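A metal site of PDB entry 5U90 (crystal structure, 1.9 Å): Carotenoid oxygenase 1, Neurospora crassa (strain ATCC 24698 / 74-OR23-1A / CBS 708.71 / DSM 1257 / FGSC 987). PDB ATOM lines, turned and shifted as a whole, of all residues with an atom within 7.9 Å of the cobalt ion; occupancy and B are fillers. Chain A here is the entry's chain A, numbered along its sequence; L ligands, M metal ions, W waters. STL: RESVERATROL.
O3 of the ligand sits at hydrogen-bond distance from ND1 of His 313 (3.4 Å). O3 of the ligand lies within hydrogen-bond range of OE2 of Glu 383 (2.7 Å).
ND1 of His 313 is in hydrogen-bond range of OE1 of Glu 383, at 2.7 Å. The side-chain hydroxyl (OG1) of Thr 195 lies within hydrogen-bond range of the backbone NH (N) of His 197 (3.1 Å). N of His 510 sits at hydrogen-bond distance from O of Thr 151, 3.1 Å away. The side-chain carboxylate (OE2) of Glu 453 sits at hydrogen-bond distance from a ring nitrogen (ND1) of His 510 (2.8 Å). A ring nitrogen (ND1) of His 248 is in hydrogen-bond range of the side-chain carboxylate of Glu 165 (2.7 Å).
Within 4 Å of the cobalt ion: His 197, His 248, His 313 and His 510.
NE2 of His 313 is bound to the cobalt ion, 2.1 Å away. NE2 of His 197 is bound to the cobalt ion (2.1 Å). The cobalt ion is bound by NE2 of His 510, 2.2 Å away. NE2 of His 248 is bound to the cobalt ion, at 2.2 Å. The cobalt ion is bound by water W1 (2.3 Å). The cobalt ion has five donor atoms within binding distance.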
ATOM      1  N   THR A 151      -4.253 -22.871 -27.747  1.00  0.00           N
ATOM      2  CA  THR A 151      -4.985 -23.238 -26.546  1.00  0.00           C
ATOM      3  C   THR A 151      -5.761 -22.112 -25.890  1.00  0.00           C
ATOM      4  O   THR A 151      -6.885 -22.332 -25.466  1.00  0.00           O
ATOM      5  CB  THR A 151      -4.002 -23.878 -25.510  1.00  0.00           C
ATOM      6  OG1 THR A 151      -3.358 -24.985 -26.140  1.00  0.00           O
ATOM      7  CG2 THR A 151      -4.773 -24.358 -24.283  1.00  0.00           C
ATOM      8  N   ASN A 152      -5.167 -20.907 -25.797  1.00  0.00           N
ATOM      9  CA  ASN A 152      -5.913 -19.750 -25.309  1.00  0.00           C
ATOM     10  C   ASN A 152      -5.454 -18.491 -26.068  1.00  0.00           C
ATOM     11  O   ASN A 152      -4.402 -18.495 -26.733  1.00  0.00           O
ATOM     12  CB  ASN A 152      -5.763 -19.588 -23.796  1.00  0.00           C
ATOM     13  CG  ASN A 152      -6.885 -18.765 -23.136  1.00  0.00           C
ATOM     14  OD1 ASN A 152      -7.764 -18.191 -23.786  1.00  0.00           O
ATOM     15  ND2 ASN A 152      -6.853 -18.699 -21.811  1.00  0.00           N
ATOM     16  N   GLU A 165       1.151 -24.195 -23.718  1.00  0.00           N
ATOM     17  CA  GLU A 165       1.876 -24.436 -22.448  1.00  0.00           C
ATOM     18  C   GLU A 165       3.301 -24.996 -22.581  1.00  0.00           C
ATOM     19  O   GLU A 165       3.996 -25.084 -21.562  1.00  0.00           O
ATOM     20  CB  GLU A 165       1.033 -25.335 -21.535  1.00  0.00           C
ATOM     21  CG  GLU A 165       0.858 -26.771 -21.997  1.00  0.00           C
ATOM     22  CD  GLU A 165      -0.341 -27.425 -21.361  1.00  0.00           C
ATOM     23  OE1 GLU A 165      -0.139 -28.536 -20.738  1.00  0.00           O
ATOM     24  OE2 GLU A 165      -1.463 -26.887 -21.473  1.00  0.00           O
ATOM     25  N   THR A 195       2.028 -20.698 -19.350  1.00  0.00           N
ATOM     26  CA  THR A 195       0.770 -21.422 -19.209  1.00  0.00           C
ATOM     27  C   THR A 195      -0.318 -20.858 -20.151  1.00  0.00           C
ATOM     28  O   THR A 195      -0.347 -19.653 -20.467  1.00  0.00           O
ATOM     29  CB  THR A 195       0.259 -21.318 -17.764  1.00  0.00           C
ATOM     30  OG1 THR A 195      -0.953 -22.055 -17.576  1.00  0.00           O
ATOM     31  CG2 THR A 195      -0.014 -19.870 -17.348  1.00  0.00           C
ATOM     32  N   ALA A 196      -1.254 -21.715 -20.533  1.00  0.00           N
ATOM     33  CA  ALA A 196      -2.419 -21.245 -21.233  1.00  0.00           C
ATOM     34  C   ALA A 196      -3.442 -20.591 -20.336  1.00  0.00           C
ATOM     35  O   ALA A 196      -4.423 -20.105 -20.843  1.00  0.00           O
ATOM     36  CB  ALA A 196      -3.062 -22.394 -21.987  1.00  0.00           C
ATOM     37  N   HIS A 197      -3.246 -20.634 -19.012  1.00  0.00           N
ATOM     38  CA  HIS A 197      -4.225 -20.091 -18.074  1.00  0.00           C
ATOM     39  C   HIS A 197      -3.655 -19.058 -17.084  1.00  0.00           C
ATOM     40  O   HIS A 197      -3.777 -19.217 -15.886  1.00  0.00           O
ATOM     41  CB  HIS A 197      -4.924 -21.223 -17.354  1.00  0.00           C
ATOM     42  CG  HIS A 197      -5.794 -22.034 -18.249  1.00  0.00           C
ATOM     43  ND1 HIS A 197      -6.980 -21.528 -18.733  1.00  0.00           N
ATOM     44  CD2 HIS A 197      -5.619 -23.238 -18.840  1.00  0.00           C
ATOM     45  CE1 HIS A 197      -7.526 -22.402 -19.559  1.00  0.00           C
ATOM     46  NE2 HIS A 197      -6.715 -23.453 -19.637  1.00  0.00           N
ATOM     47  N   HIS A 248      -1.889 -28.101 -16.322  1.00  0.00           N
ATOM     48  CA  HIS A 248      -2.582 -27.386 -17.373  1.00  0.00           C
ATOM     49  C   HIS A 248      -3.163 -26.033 -16.932  1.00  0.00           C
ATOM     50  O   HIS A 248      -3.148 -25.054 -17.695  1.00  0.00           O
ATOM     51  CB  HIS A 248      -3.723 -28.221 -17.915  1.00  0.00           C
ATOM     52  CG  HIS A 248      -4.425 -27.545 -19.026  1.00  0.00           C
ATOM     53  ND1 HIS A 248      -3.768 -27.236 -20.198  1.00  0.00           N
ATOM     54  CD2 HIS A 248      -5.658 -27.021 -19.131  1.00  0.00           C
ATOM     55  CE1 HIS A 248      -4.571 -26.555 -20.989  1.00  0.00           C
ATOM     56  NE2 HIS A 248      -5.726 -26.429 -20.373  1.00  0.00           N
ATOM     57  N   ASP A 249      -3.678 -26.010 -15.714  1.00  0.00           N
ATOM     58  CA  ASP A 249      -4.343 -24.820 -15.155  1.00  0.00           C
ATOM     59  C   ASP A 249      -3.780 -24.613 -13.754  1.00  0.00           C
ATOM     60  O   ASP A 249      -3.070 -25.488 -13.229  1.00  0.00           O
ATOM     61  CB  ASP A 249      -5.861 -25.050 -15.123  1.00  0.00           C
ATOM     62  CG  ASP A 249      -6.681 -23.752 -15.084  1.00  0.00           C
ATOM     63  OD1 ASP A 249      -6.152 -22.646 -14.823  1.00  0.00           O
ATOM     64  OD2 ASP A 249      -7.898 -23.852 -15.304  1.00  0.00           O
ATOM     65  N   GLY A 312      -8.956 -31.010 -13.684  1.00  0.00           N
ATOM     66  CA  GLY A 312      -9.602 -30.258 -14.777  1.00  0.00           C
ATOM     67  C   GLY A 312      -9.536 -28.749 -14.557  1.00  0.00           C
ATOM     68  O   GLY A 312      -8.826 -28.288 -13.684  1.00  0.00           O
ATOM     69  N   HIS A 313     -10.289 -27.982 -15.349  1.00  0.00           N
ATOM     70  CA  HIS A 313     -10.171 -26.529 -15.272  1.00  0.00           C
ATOM     71  C   HIS A 313     -10.612 -25.927 -13.950  1.00  0.00           C
ATOM     72  O   HIS A 313     -11.582 -26.376 -13.324  1.00  0.00           O
ATOM     73  CB  HIS A 313     -10.904 -25.854 -16.411  1.00  0.00           C
ATOM     74  CG  HIS A 313     -10.220 -26.018 -17.715  1.00  0.00           C
ATOM     75  ND1 HIS A 313     -10.642 -26.897 -18.695  1.00  0.00           N
ATOM     76  CD2 HIS A 313      -9.095 -25.432 -18.195  1.00  0.00           C
ATOM     77  CE1 HIS A 313      -9.829 -26.821 -19.731  1.00  0.00           C
ATOM     78  NE2 HIS A 313      -8.882 -25.947 -19.449  1.00  0.00           N
ATOM     79  N   VAL A 314      -9.876 -24.905 -13.543  1.00  0.00           N
ATOM     80  CA  VAL A 314     -10.207 -24.127 -12.362  1.00  0.00           C
ATOM     81  C   VAL A 314     -11.280 -23.071 -12.679  1.00  0.00           C
ATOM     82  O   VAL A 314     -11.141 -22.281 -13.590  1.00  0.00           O
ATOM     83  CB  VAL A 314      -8.956 -23.433 -11.810  1.00  0.00           C
ATOM     84  CG1 VAL A 314      -9.306 -22.522 -10.635  1.00  0.00           C
ATOM     85  CG2 VAL A 314      -7.897 -24.485 -11.417  1.00  0.00           C
ATOM     86  N   PHE A 337      -7.759 -37.769 -20.619  1.00  0.00           N
ATOM     87  CA  PHE A 337      -7.000 -37.853 -21.846  1.00  0.00           C
ATOM     88  C   PHE A 337      -6.584 -39.315 -22.078  1.00  0.00           C
ATOM     89  O   PHE A 337      -5.393 -39.698 -22.057  1.00  0.00           O
ATOM     90  CB  PHE A 337      -5.772 -36.908 -21.822  1.00  0.00           C
ATOM     91  CG  PHE A 337      -6.072 -35.442 -21.556  1.00  0.00           C
ATOM     92  CD1 PHE A 337      -7.338 -34.894 -21.691  1.00  0.00           C
ATOM     93  CD2 PHE A 337      -5.029 -34.613 -21.187  1.00  0.00           C
ATOM     94  CE1 PHE A 337      -7.558 -33.534 -21.419  1.00  0.00           C
ATOM     95  CE2 PHE A 337      -5.229 -33.256 -20.923  1.00  0.00           C
ATOM     96  CZ  PHE A 337      -6.499 -32.721 -21.052  1.00  0.00           C
ATOM     97  N   GLU A 383     -17.465 -29.189 -17.426  1.00  0.00           N
ATOM     98  CA  GLU A 383     -16.116 -28.650 -17.676  1.00  0.00           C
ATOM     99  C   GLU A 383     -16.233 -27.209 -18.179  1.00  0.00           C
ATOM    100  O   GLU A 383     -17.360 -26.650 -18.284  1.00  0.00           O
ATOM    101  CB  GLU A 383     -15.299 -29.525 -18.673  1.00  0.00           C
ATOM    102  CG  GLU A 383     -14.150 -30.300 -18.017  1.00  0.00           C
ATOM    103  CD  GLU A 383     -12.924 -29.492 -17.655  1.00  0.00           C
ATOM    104  OE1 GLU A 383     -12.890 -28.245 -17.878  1.00  0.00           O
ATOM    105  OE2 GLU A 383     -11.927 -30.117 -17.154  1.00  0.00           O
ATOM    106  N   PHE A 384     -15.083 -26.603 -18.440  1.00  0.00           N
ATOM    107  CA  PHE A 384     -14.954 -25.254 -18.987  1.00  0.00           C
ATOM    108  C   PHE A 384     -15.735 -24.211 -18.190  1.00  0.00           C
ATOM    109  O   PHE A 384     -16.572 -23.498 -18.747  1.00  0.00           O
ATOM    110  CB  PHE A 384     -15.349 -25.265 -20.488  1.00  0.00           C
ATOM    111  CG  PHE A 384     -14.816 -26.464 -21.217  1.00  0.00           C
ATOM    112  CD1 PHE A 384     -13.444 -26.748 -21.190  1.00  0.00           C
ATOM    113  CD2 PHE A 384     -15.690 -27.342 -21.878  1.00  0.00           C
ATOM    114  CE1 PHE A 384     -12.957 -27.884 -21.849  1.00  0.00           C
ATOM    115  CE2 PHE A 384     -15.209 -28.460 -22.498  1.00  0.00           C
ATOM    116  CZ  PHE A 384     -13.840 -28.725 -22.486  1.00  0.00           C
ATOM    117  N   GLU A 453     -16.869 -23.595 -25.130  1.00  0.00           N
ATOM    118  CA  GLU A 453     -16.727 -22.815 -23.904  1.00  0.00           C
ATOM    119  C   GLU A 453     -17.378 -21.457 -24.071  1.00  0.00           C
ATOM    120  O   GLU A 453     -17.193 -20.800 -25.100  1.00  0.00           O
ATOM    121  CB  GLU A 453     -15.234 -22.599 -23.577  1.00  0.00           C
ATOM    122  CG  GLU A 453     -14.991 -21.712 -22.356  1.00  0.00           C
ATOM    123  CD  GLU A 453     -13.545 -21.262 -22.241  1.00  0.00           C
ATOM    124  OE1 GLU A 453     -13.085 -20.518 -23.121  1.00  0.00           O
ATOM    125  OE2 GLU A 453     -12.847 -21.633 -21.276  1.00  0.00           O
ATOM    126  N   LEU A 509     -10.736 -24.496 -28.312  1.00  0.00           N
ATOM    127  CA  LEU A 509     -10.325 -24.490 -26.940  1.00  0.00           C
ATOM    128  C   LEU A 509     -10.829 -23.196 -26.344  1.00  0.00           C
ATOM    129  O   LEU A 509     -12.067 -22.979 -26.339  1.00  0.00           O
ATOM    130  CB  LEU A 509      -8.823 -24.751 -26.826  1.00  0.00           C
ATOM    131  CG  LEU A 509      -8.456 -26.216 -27.144  1.00  0.00           C
ATOM    132  CD1 LEU A 509      -6.985 -26.438 -27.379  1.00  0.00           C
ATOM    133  CD2 LEU A 509      -8.943 -27.123 -26.027  1.00  0.00           C
ATOM    134  N   HIS A 510      -9.966 -22.343 -25.825  1.00  0.00           N
ATOM    135  CA  HIS A 510     -10.439 -21.254 -24.964  1.00  0.00           C
ATOM    136  C   HIS A 510     -10.721 -19.970 -25.743  1.00  0.00           C
ATOM    137  O   HIS A 510     -10.272 -19.833 -26.889  1.00  0.00           O
ATOM    138  CB  HIS A 510      -9.459 -21.015 -23.832  1.00  0.00           C
ATOM    139  CG  HIS A 510      -9.352 -22.168 -22.917  1.00  0.00           C
ATOM    140  ND1 HIS A 510     -10.381 -22.540 -22.088  1.00  0.00           N
ATOM    141  CD2 HIS A 510      -8.390 -23.113 -22.773  1.00  0.00           C
ATOM    142  CE1 HIS A 510     -10.038 -23.636 -21.443  1.00  0.00           C
ATOM    143  NE2 HIS A 510      -8.850 -24.006 -21.864  1.00  0.00           N
HETATM  144  C1  STL L   1      -9.419 -30.017 -19.583  1.00  0.00           C
HETATM  145  C2  STL L   1     -10.561 -30.499 -20.230  1.00  0.00           C
HETATM  146  C3  STL L   1     -10.578 -30.561 -21.626  1.00  0.00           C
HETATM  147  C4  STL L   1      -9.496 -30.144 -22.363  1.00  0.00           C
HETATM  148  C5  STL L   1      -8.336 -29.674 -21.728  1.00  0.00           C
HETATM  149  C6  STL L   1      -8.305 -29.597 -20.324  1.00  0.00           C
HETATM  150  C7  STL L   1      -7.182 -29.377 -22.607  1.00  0.00           C
HETATM  151  C8  STL L   1      -5.965 -29.289 -22.282  1.00  0.00           C
HETATM  152  C9  STL L   1      -4.821 -29.027 -23.175  1.00  0.00           C
HETATM  153  C10 STL L   1      -4.957 -28.486 -24.461  1.00  0.00           C
HETATM  154  C11 STL L   1      -3.858 -28.348 -25.301  1.00  0.00           C
HETATM  155  C12 STL L   1      -2.597 -28.735 -24.856  1.00  0.00           C
HETATM  156  C13 STL L   1      -2.450 -29.242 -23.578  1.00  0.00           C
HETATM  157  C14 STL L   1      -3.558 -29.379 -22.760  1.00  0.00           C
HETATM  158  O1  STL L   1      -1.510 -28.658 -25.678  1.00  0.00           O
HETATM  159  O2  STL L   1     -11.655 -31.071 -22.281  1.00  0.00           O
HETATM  160  O3  STL L   1      -9.408 -29.972 -18.195  1.00  0.00           O
HETATM  161 CO    CO M   1      -7.442 -25.113 -20.667  1.00  0.00          CO
HETATM  162  O   HOH W   1      -7.640 -26.249 -22.670  1.00  0.00           O
